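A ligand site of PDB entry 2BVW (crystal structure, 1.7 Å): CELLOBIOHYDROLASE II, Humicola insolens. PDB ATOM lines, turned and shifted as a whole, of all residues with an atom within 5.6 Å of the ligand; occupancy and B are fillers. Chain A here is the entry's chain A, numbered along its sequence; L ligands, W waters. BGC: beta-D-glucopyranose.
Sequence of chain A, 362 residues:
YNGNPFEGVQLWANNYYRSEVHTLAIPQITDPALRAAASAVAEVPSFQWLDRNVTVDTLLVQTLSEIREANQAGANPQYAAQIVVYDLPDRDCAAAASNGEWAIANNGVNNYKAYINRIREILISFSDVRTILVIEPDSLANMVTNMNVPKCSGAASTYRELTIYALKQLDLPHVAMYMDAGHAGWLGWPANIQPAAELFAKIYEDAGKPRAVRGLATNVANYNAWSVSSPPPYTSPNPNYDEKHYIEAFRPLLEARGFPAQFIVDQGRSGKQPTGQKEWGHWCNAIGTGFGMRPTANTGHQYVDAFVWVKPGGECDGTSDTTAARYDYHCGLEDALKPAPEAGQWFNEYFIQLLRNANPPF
Water W3 lies within hydrogen-bond range of an oxygen (O1) of the ligand (2.7 Å), the side-chain hydroxyl of Tyr 86 (2.9 Å) and the side-chain hydroxyl of Ser 98 (3.4 Å).
Water W4 lies within hydrogen-bond range of OD1 of Asp 317 (2.7 Å), O1 of the ligand (2.8 Å) and NZ of Lys 311 (2.8 Å).
Water W1 lies within hydrogen-bond range of an oxygen (O2) of the ligand (2.8 Å), the guanidinium group (NH1) of Arg 326 (2.9 Å), the backbone carbonyl oxygen (O) of Ala 343 (3.5 Å) and the guanidinium group (NH2) of Arg 91 (3.5 Å).
Water W2 lies within hydrogen-bond range of OE1 of Glu 315 (2.8 Å) and O4 of the ligand (2.8 Å).
O6 of the ligand is in hydrogen-bond range of OE1 of Glu 315, 2.7 Å away.
The side-chain hydroxyl of Ser 98 lies within hydrogen-bond range of an oxygen (O2) of the ligand (2.8 Å).
OD2 of Asp 51 lies within hydrogen-bond range of O3 of the ligand, at 2.9 Å.
The side-chain amino group (NZ) of Lys 311 sits at hydrogen-bond distance from an oxygen (O6) of the ligand, 2.9 Å away.
Residues that only touch the ligand: Trp 49, Tyr 86, Arg 91, Pro 312, Ala 343 and Gly 344.
Hydrophobic or aromatic side chains that line the ligand: Trp 49, Tyr 86, Pro 312 and Ala 343.
The nearest printed residue that does not touch the ligand is Cys 316 (4.3 Å).
The side-chain amino group (NZ) of Lys 311 lies within hydrogen-bond range of the backbone carbonyl oxygen (O) of Glu 315, 3.0 Å away.
O of Ser 98 sits at hydrogen-bond distance from NE of Arg 91 (2.9 Å).
O of Asp 51 sits at hydrogen-bond distance from NH1 of Arg 91 (2.9 Å).
The side-chain amino group (NZ) of Lys 311 is in hydrogen-bond range of the backbone carbonyl oxygen (O) of Cys 316, 3.1 Å away.
The side-chain amino group of Lys 311 lies within salt-bridge range of the side-chain carboxylate of Asp 317 (3.5 Å).
The backbone carbonyl oxygen (O) of Cys 316 sits at hydrogen-bond distance from the backbone NH (N) of Gly 344 (2.8 Å).
NH1 of Arg 91 sits at hydrogen-bond distance from O of Tyr 86 (2.9 Å).
NH2 of Arg 326 is in hydrogen-bond range of O of Ala 343, at 3.5 Å.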
ATOM      1  N   TRP A  49       0.947 -24.980  -9.183  1.00  0.00           N
ATOM      2  CA  TRP A  49       1.653 -23.776  -9.610  1.00  0.00           C
ATOM      3  C   TRP A  49       2.787 -24.034 -10.582  1.00  0.00           C
ATOM      4  O   TRP A  49       3.683 -24.868 -10.336  1.00  0.00           O
ATOM      5  CB  TRP A  49       2.211 -23.082  -8.349  1.00  0.00           C
ATOM      6  CG  TRP A  49       1.148 -22.450  -7.498  1.00  0.00           C
ATOM      7  CD1 TRP A  49       0.075 -23.075  -6.904  1.00  0.00           C
ATOM      8  CD2 TRP A  49       1.075 -21.077  -7.105  1.00  0.00           C
ATOM      9  NE1 TRP A  49      -0.655 -22.140  -6.184  1.00  0.00           N
ATOM     10  CE2 TRP A  49      -0.055 -20.924  -6.299  1.00  0.00           C
ATOM     11  CE3 TRP A  49       1.882 -19.971  -7.398  1.00  0.00           C
ATOM     12  CZ2 TRP A  49      -0.448 -19.677  -5.785  1.00  0.00           C
ATOM     13  CZ3 TRP A  49       1.518 -18.746  -6.856  1.00  0.00           C
ATOM     14  CH2 TRP A  49       0.383 -18.601  -6.030  1.00  0.00           C
ATOM     15  N   ASP A  51       5.548 -22.380 -11.066  1.00  0.00           N
ATOM     16  CA  ASP A  51       6.381 -21.338 -10.491  1.00  0.00           C
ATOM     17  C   ASP A  51       7.784 -21.270 -11.045  1.00  0.00           C
ATOM     18  O   ASP A  51       8.563 -20.381 -10.730  1.00  0.00           O
ATOM     19  CB  ASP A  51       6.423 -21.485  -8.949  1.00  0.00           C
ATOM     20  CG  ASP A  51       7.240 -22.713  -8.533  1.00  0.00           C
ATOM     21  OD1 ASP A  51       6.988 -23.839  -9.029  1.00  0.00           O
ATOM     22  OD2 ASP A  51       8.139 -22.575  -7.679  1.00  0.00           O
ATOM     23  N   TYR A  86       2.830 -18.496 -12.907  1.00  0.00           N
ATOM     24  CA  TYR A  86       3.538 -17.602 -11.948  1.00  0.00           C
ATOM     25  C   TYR A  86       5.028 -17.543 -12.161  1.00  0.00           C
ATOM     26  O   TYR A  86       5.763 -18.214 -11.417  1.00  0.00           O
ATOM     27  CB  TYR A  86       3.226 -18.128 -10.535  1.00  0.00           C
ATOM     28  CG  TYR A  86       3.733 -17.280  -9.387  1.00  0.00           C
ATOM     29  CD1 TYR A  86       3.361 -15.945  -9.242  1.00  0.00           C
ATOM     30  CD2 TYR A  86       4.605 -17.801  -8.429  1.00  0.00           C
ATOM     31  CE1 TYR A  86       3.811 -15.154  -8.191  1.00  0.00           C
ATOM     32  CE2 TYR A  86       5.060 -17.035  -7.367  1.00  0.00           C
ATOM     33  CZ  TYR A  86       4.669 -15.715  -7.268  1.00  0.00           C
ATOM     34  OH  TYR A  86       5.152 -14.947  -6.213  1.00  0.00           O
ATOM     35  N   ARG A  91       9.613 -10.901 -10.670  1.00  0.00           N
ATOM     36  CA  ARG A  91       8.427 -11.350  -9.952  1.00  0.00           C
ATOM     37  C   ARG A  91       8.421 -10.833  -8.526  1.00  0.00           C
ATOM     38  O   ARG A  91       9.470 -10.485  -7.970  1.00  0.00           O
ATOM     39  CB  ARG A  91       8.456 -12.896  -9.926  1.00  0.00           C
ATOM     40  CG  ARG A  91       7.118 -13.530  -9.599  1.00  0.00           C
ATOM     41  CD  ARG A  91       7.204 -15.078  -9.778  1.00  0.00           C
ATOM     42  NE  ARG A  91       8.000 -15.602  -8.656  1.00  0.00           N
ATOM     43  CZ  ARG A  91       8.315 -16.906  -8.584  1.00  0.00           C
ATOM     44  NH1 ARG A  91       7.925 -17.795  -9.502  1.00  0.00           N
ATOM     45  NH2 ARG A  91       9.038 -17.326  -7.556  1.00  0.00           N
ATOM     46  N   ALA A  97      10.637 -12.416  -0.759  1.00  0.00           N
ATOM     47  CA  ALA A  97      10.480 -13.841  -0.501  1.00  0.00           C
ATOM     48  C   ALA A  97      10.245 -14.744  -1.699  1.00  0.00           C
ATOM     49  O   ALA A  97      10.734 -15.899  -1.701  1.00  0.00           O
ATOM     50  CB  ALA A  97       9.331 -14.044   0.486  1.00  0.00           C
ATOM     51  N   SER A  98       9.477 -14.253  -2.664  1.00  0.00           N
ATOM     52  CA  SER A  98       9.164 -15.055  -3.844  1.00  0.00           C
ATOM     53  C   SER A  98       9.785 -14.540  -5.121  1.00  0.00           C
ATOM     54  O   SER A  98       9.224 -14.697  -6.217  1.00  0.00           O
ATOM     55  CB  SER A  98       7.654 -15.277  -3.971  1.00  0.00           C
ATOM     56  OG  SER A  98       7.218 -16.203  -2.956  1.00  0.00           O
ATOM     57  N   LYS A 311      -3.545 -21.100  -3.126  1.00  0.00           N
ATOM     58  CA  LYS A 311      -2.249 -21.331  -2.450  1.00  0.00           C
ATOM     59  C   LYS A 311      -2.373 -22.644  -1.676  1.00  0.00           C
ATOM     60  O   LYS A 311      -3.299 -22.802  -0.874  1.00  0.00           O
ATOM     61  CB  LYS A 311      -2.015 -20.185  -1.475  1.00  0.00           C
ATOM     62  CG  LYS A 311      -0.896 -20.487  -0.470  1.00  0.00           C
ATOM     63  CD  LYS A 311       0.474 -20.481  -1.107  1.00  0.00           C
ATOM     64  CE  LYS A 311       1.559 -20.803  -0.079  1.00  0.00           C
ATOM     65  NZ  LYS A 311       2.925 -20.653  -0.622  1.00  0.00           N
ATOM     66  N   PRO A 312      -1.515 -23.617  -1.934  1.00  0.00           N
ATOM     67  CA  PRO A 312      -1.602 -24.927  -1.269  1.00  0.00           C
ATOM     68  C   PRO A 312      -1.026 -24.835   0.141  1.00  0.00           C
ATOM     69  O   PRO A 312       0.181 -24.665   0.315  1.00  0.00           O
ATOM     70  CB  PRO A 312      -0.853 -25.871  -2.231  1.00  0.00           C
ATOM     71  CG  PRO A 312      -0.601 -25.051  -3.464  1.00  0.00           C
ATOM     72  CD  PRO A 312      -0.444 -23.631  -2.945  1.00  0.00           C
ATOM     73  N   GLU A 315       2.706 -25.176   1.943  1.00  0.00           N
ATOM     74  CA  GLU A 315       3.802 -24.675   1.125  1.00  0.00           C
ATOM     75  C   GLU A 315       4.141 -23.275   1.665  1.00  0.00           C
ATOM     76  O   GLU A 315       3.282 -22.399   1.739  1.00  0.00           O
ATOM     77  CB  GLU A 315       3.496 -24.667  -0.371  1.00  0.00           C
ATOM     78  CG  GLU A 315       3.436 -26.137  -0.846  1.00  0.00           C
ATOM     79  CD  GLU A 315       3.037 -26.245  -2.298  1.00  0.00           C
ATOM     80  OE1 GLU A 315       3.013 -25.221  -3.029  1.00  0.00           O
ATOM     81  OE2 GLU A 315       2.788 -27.391  -2.747  1.00  0.00           O
ATOM     82  N   CYS A 316       5.378 -23.083   2.074  1.00  0.00           N
ATOM     83  CA  CYS A 316       5.832 -21.845   2.695  1.00  0.00           C
ATOM     84  C   CYS A 316       5.653 -20.572   1.884  1.00  0.00           C
ATOM     85  O   CYS A 316       5.716 -20.593   0.646  1.00  0.00           O
ATOM     86  CB  CYS A 316       7.327 -22.025   3.039  1.00  0.00           C
ATOM     87  SG  CYS A 316       7.845 -20.856   4.327  1.00  0.00           S
ATOM     88  N   ASP A 317       5.489 -19.461   2.628  1.00  0.00           N
ATOM     89  CA  ASP A 317       5.408 -18.163   1.991  1.00  0.00           C
ATOM     90  C   ASP A 317       6.769 -17.467   1.884  1.00  0.00           C
ATOM     91  O   ASP A 317       6.895 -16.461   1.173  1.00  0.00           O
ATOM     92  CB  ASP A 317       4.469 -17.178   2.720  1.00  0.00           C
ATOM     93  CG  ASP A 317       3.060 -17.699   2.822  1.00  0.00           C
ATOM     94  OD1 ASP A 317       2.564 -18.192   1.783  1.00  0.00           O
ATOM     95  OD2 ASP A 317       2.449 -17.622   3.894  1.00  0.00           O
ATOM     96  N   ARG A 326      16.666 -14.269  -0.316  1.00  0.00           N
ATOM     97  CA  ARG A 326      15.260 -13.949  -0.393  1.00  0.00           C
ATOM     98  C   ARG A 326      14.602 -13.640   0.931  1.00  0.00           C
ATOM     99  O   ARG A 326      13.383 -13.676   1.037  1.00  0.00           O
ATOM    100  CB  ARG A 326      14.502 -15.078  -1.123  1.00  0.00           C
ATOM    101  CG  ARG A 326      14.974 -15.301  -2.552  1.00  0.00           C
ATOM    102  CD  ARG A 326      13.908 -15.976  -3.415  1.00  0.00           C
ATOM    103  NE  ARG A 326      13.492 -17.247  -2.825  1.00  0.00           N
ATOM    104  CZ  ARG A 326      12.486 -17.966  -3.344  1.00  0.00           C
ATOM    105  NH1 ARG A 326      11.862 -17.562  -4.437  1.00  0.00           N
ATOM    106  NH2 ARG A 326      12.126 -19.091  -2.764  1.00  0.00           N
ATOM    107  N   ALA A 343      10.322 -19.952   0.296  1.00  0.00           N
ATOM    108  CA  ALA A 343       8.970 -19.885  -0.244  1.00  0.00           C
ATOM    109  C   ALA A 343       8.757 -21.051  -1.222  1.00  0.00           C
ATOM    110  O   ALA A 343       9.628 -21.381  -2.020  1.00  0.00           O
ATOM    111  CB  ALA A 343       8.778 -18.579  -1.004  1.00  0.00           C
ATOM    112  N   GLY A 344       7.606 -21.705  -1.031  1.00  0.00           N
ATOM    113  CA  GLY A 344       7.272 -22.824  -1.890  1.00  0.00           C
ATOM    114  C   GLY A 344       7.751 -24.159  -1.374  1.00  0.00           C
ATOM    115  O   GLY A 344       7.260 -25.198  -1.848  1.00  0.00           O
HETATM  116  C2  BGC L   1       6.162 -19.552  -4.073  1.00  0.00           C
HETATM  117  C3  BGC L   1       6.082 -20.621  -5.157  1.00  0.00           C
HETATM  118  C4  BGC L   1       4.967 -21.621  -4.861  1.00  0.00           C
HETATM  119  C5  BGC L   1       3.602 -20.967  -4.567  1.00  0.00           C
HETATM  120  C6  BGC L   1       2.602 -21.984  -4.042  1.00  0.00           C
HETATM  121  C1  BGC L   1       4.735 -18.989  -3.821  1.00  0.00           C
HETATM  122  O1  BGC L   1       4.774 -18.109  -2.726  1.00  0.00           O
HETATM  123  O2  BGC L   1       7.079 -18.517  -4.457  1.00  0.00           O
HETATM  124  O3  BGC L   1       7.346 -21.285  -5.217  1.00  0.00           O
HETATM  125  O4  BGC L   1       4.886 -22.494  -5.999  1.00  0.00           O
HETATM  126  O5  BGC L   1       3.784 -19.995  -3.483  1.00  0.00           O
HETATM  127  O6  BGC L   1       2.963 -22.578  -2.778  1.00  0.00           O
HETATM  128  O   HOH W   1       9.725 -19.427  -4.883  1.00  0.00           O
HETATM  129  O   HOH W   2       3.856 -25.117  -5.645  1.00  0.00           O
HETATM  130  O   HOH W   3       3.929 -15.706  -3.687  1.00  0.00           O
HETATM  131  O   HOH W   4       2.704 -17.856  -0.931  1.00  0.00           O
